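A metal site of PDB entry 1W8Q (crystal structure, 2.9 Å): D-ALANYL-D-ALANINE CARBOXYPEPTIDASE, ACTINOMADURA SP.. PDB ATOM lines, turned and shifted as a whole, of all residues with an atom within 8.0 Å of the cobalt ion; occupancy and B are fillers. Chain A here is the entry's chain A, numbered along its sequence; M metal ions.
Ala 186 touches the cobalt ion.
Of the 12 residues printed, 4 come within 4 Å of the cobalt ion.
The nearest printed residue that does not touch the cobalt ion is Gly 189 (4.1 Å).
The cobalt ion is bound by OE1 of Glu 251 (2.0 Å), O of Glu 188 (2.0 Å) and NE2 of His 247 (2.2 Å).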
ATOM      1  N   GLY A 185      33.119 -26.074 -14.390  1.00  0.00           N
ATOM      2  CA  GLY A 185      32.193 -26.274 -15.481  1.00  0.00           C
ATOM      3  C   GLY A 185      31.615 -24.950 -15.939  1.00  0.00           C
ATOM      4  O   GLY A 185      32.335 -23.953 -16.060  1.00  0.00           O
ATOM      5  N   ALA A 186      30.305 -24.935 -16.192  1.00  0.00           N
ATOM      6  CA  ALA A 186      29.629 -23.734 -16.670  1.00  0.00           C
ATOM      7  C   ALA A 186      29.793 -22.537 -15.745  1.00  0.00           C
ATOM      8  O   ALA A 186      29.958 -21.413 -16.214  1.00  0.00           O
ATOM      9  CB  ALA A 186      28.158 -24.014 -16.886  1.00  0.00           C
ATOM     10  N   ALA A 187      29.762 -22.786 -14.435  1.00  0.00           N
ATOM     11  CA  ALA A 187      29.886 -21.703 -13.450  1.00  0.00           C
ATOM     12  C   ALA A 187      31.247 -21.012 -13.443  1.00  0.00           C
ATOM     13  O   ALA A 187      31.478 -20.117 -12.630  1.00  0.00           O
ATOM     14  CB  ALA A 187      29.562 -22.235 -12.059  1.00  0.00           C
ATOM     15  N   GLU A 188      32.152 -21.432 -14.314  1.00  0.00           N
ATOM     16  CA  GLU A 188      33.474 -20.811 -14.409  1.00  0.00           C
ATOM     17  C   GLU A 188      33.306 -19.335 -14.715  1.00  0.00           C
ATOM     18  O   GLU A 188      32.632 -18.970 -15.672  1.00  0.00           O
ATOM     19  CB  GLU A 188      34.278 -21.450 -15.541  1.00  0.00           C
ATOM     20  CG  GLU A 188      35.416 -22.354 -15.126  1.00  0.00           C
ATOM     21  CD  GLU A 188      36.375 -21.685 -14.162  1.00  0.00           C
ATOM     22  OE1 GLU A 188      36.720 -20.500 -14.368  1.00  0.00           O
ATOM     23  OE2 GLU A 188      36.802 -22.372 -13.194  1.00  0.00           O
ATOM     24  N   GLY A 189      33.920 -18.474 -13.911  1.00  0.00           N
ATOM     25  CA  GLY A 189      33.815 -17.052 -14.152  1.00  0.00           C
ATOM     26  C   GLY A 189      32.546 -16.461 -13.568  1.00  0.00           C
ATOM     27  O   GLY A 189      32.371 -15.245 -13.514  1.00  0.00           O
ATOM     28  N   TYR A 190      31.662 -17.342 -13.122  1.00  0.00           N
ATOM     29  CA  TYR A 190      30.410 -16.947 -12.521  1.00  0.00           C
ATOM     30  C   TYR A 190      30.492 -17.114 -10.999  1.00  0.00           C
ATOM     31  O   TYR A 190      30.407 -16.148 -10.238  1.00  0.00           O
ATOM     32  CB  TYR A 190      29.255 -17.780 -13.072  1.00  0.00           C
ATOM     33  CG  TYR A 190      27.946 -17.436 -12.423  1.00  0.00           C
ATOM     34  CD1 TYR A 190      27.302 -16.242 -12.728  1.00  0.00           C
ATOM     35  CD2 TYR A 190      27.402 -18.254 -11.443  1.00  0.00           C
ATOM     36  CE1 TYR A 190      26.153 -15.869 -12.071  1.00  0.00           C
ATOM     37  CE2 TYR A 190      26.254 -17.885 -10.772  1.00  0.00           C
ATOM     38  CZ  TYR A 190      25.633 -16.688 -11.092  1.00  0.00           C
ATOM     39  OH  TYR A 190      24.494 -16.277 -10.425  1.00  0.00           O
ATOM     40  N   ALA A 191      30.647 -18.357 -10.549  1.00  0.00           N
ATOM     41  CA  ALA A 191      30.742 -18.656  -9.125  1.00  0.00           C
ATOM     42  C   ALA A 191      32.175 -18.529  -8.660  1.00  0.00           C
ATOM     43  O   ALA A 191      33.107 -18.656  -9.447  1.00  0.00           O
ATOM     44  CB  ALA A 191      30.228 -20.056  -8.841  1.00  0.00           C
ATOM     45  N   LEU A 244      23.292 -17.188 -14.343  1.00  0.00           N
ATOM     46  CA  LEU A 244      24.229 -18.127 -14.963  1.00  0.00           C
ATOM     47  C   LEU A 244      23.880 -18.278 -16.435  1.00  0.00           C
ATOM     48  O   LEU A 244      24.781 -18.383 -17.281  1.00  0.00           O
ATOM     49  CB  LEU A 244      24.179 -19.487 -14.271  1.00  0.00           C
ATOM     50  CG  LEU A 244      25.029 -20.578 -14.939  1.00  0.00           C
ATOM     51  CD1 LEU A 244      26.500 -20.222 -14.842  1.00  0.00           C
ATOM     52  CD2 LEU A 244      24.769 -21.921 -14.286  1.00  0.00           C
ATOM     53  N   HIS A 247      25.352 -15.439 -18.008  1.00  0.00           N
ATOM     54  CA  HIS A 247      26.805 -15.558 -18.085  1.00  0.00           C
ATOM     55  C   HIS A 247      27.209 -16.421 -19.270  1.00  0.00           C
ATOM     56  O   HIS A 247      28.129 -16.075 -20.014  1.00  0.00           O
ATOM     57  CB  HIS A 247      27.349 -16.187 -16.808  1.00  0.00           C
ATOM     58  CG  HIS A 247      28.820 -16.450 -16.855  1.00  0.00           C
ATOM     59  ND1 HIS A 247      29.754 -15.532 -16.427  1.00  0.00           N
ATOM     60  CD2 HIS A 247      29.519 -17.488 -17.351  1.00  0.00           C
ATOM     61  CE1 HIS A 247      30.969 -15.992 -16.657  1.00  0.00           C
ATOM     62  NE2 HIS A 247      30.852 -17.184 -17.218  1.00  0.00           N
ATOM     63  N   LEU A 248      26.530 -17.556 -19.446  1.00  0.00           N
ATOM     64  CA  LEU A 248      26.842 -18.460 -20.544  1.00  0.00           C
ATOM     65  C   LEU A 248      26.458 -17.875 -21.909  1.00  0.00           C
ATOM     66  O   LEU A 248      27.090 -18.182 -22.917  1.00  0.00           O
ATOM     67  CB  LEU A 248      26.101 -19.788 -20.357  1.00  0.00           C
ATOM     68  CG  LEU A 248      26.500 -20.675 -19.174  1.00  0.00           C
ATOM     69  CD1 LEU A 248      25.572 -21.876 -19.118  1.00  0.00           C
ATOM     70  CD2 LEU A 248      27.942 -21.130 -19.332  1.00  0.00           C
ATOM     71  N   GLU A 250      26.513 -14.743 -22.463  1.00  0.00           N
ATOM     72  CA  GLU A 250      27.533 -13.695 -22.560  1.00  0.00           C
ATOM     73  C   GLU A 250      28.718 -14.307 -23.314  1.00  0.00           C
ATOM     74  O   GLU A 250      29.229 -13.719 -24.268  1.00  0.00           O
ATOM     75  CB  GLU A 250      27.955 -13.276 -21.150  1.00  0.00           C
ATOM     76  CG  GLU A 250      29.379 -12.723 -21.025  1.00  0.00           C
ATOM     77  CD  GLU A 250      29.483 -11.276 -21.450  1.00  0.00           C
ATOM     78  OE1 GLU A 250      29.105 -10.980 -22.602  1.00  0.00           O
ATOM     79  OE2 GLU A 250      29.950 -10.448 -20.634  1.00  0.00           O
ATOM     80  N   GLU A 251      29.140 -15.481 -22.864  1.00  0.00           N
ATOM     81  CA  GLU A 251      30.245 -16.201 -23.480  1.00  0.00           C
ATOM     82  C   GLU A 251      29.872 -16.738 -24.849  1.00  0.00           C
ATOM     83  O   GLU A 251      30.719 -16.845 -25.729  1.00  0.00           O
ATOM     84  CB  GLU A 251      30.684 -17.356 -22.568  1.00  0.00           C
ATOM     85  CG  GLU A 251      31.600 -16.928 -21.436  1.00  0.00           C
ATOM     86  CD  GLU A 251      31.697 -17.980 -20.340  1.00  0.00           C
ATOM     87  OE1 GLU A 251      32.653 -17.903 -19.535  1.00  0.00           O
ATOM     88  OE2 GLU A 251      30.821 -18.875 -20.277  1.00  0.00           O
HETATM   89 CO    CO M   1      32.379 -18.742 -17.689  1.00  0.00          CO
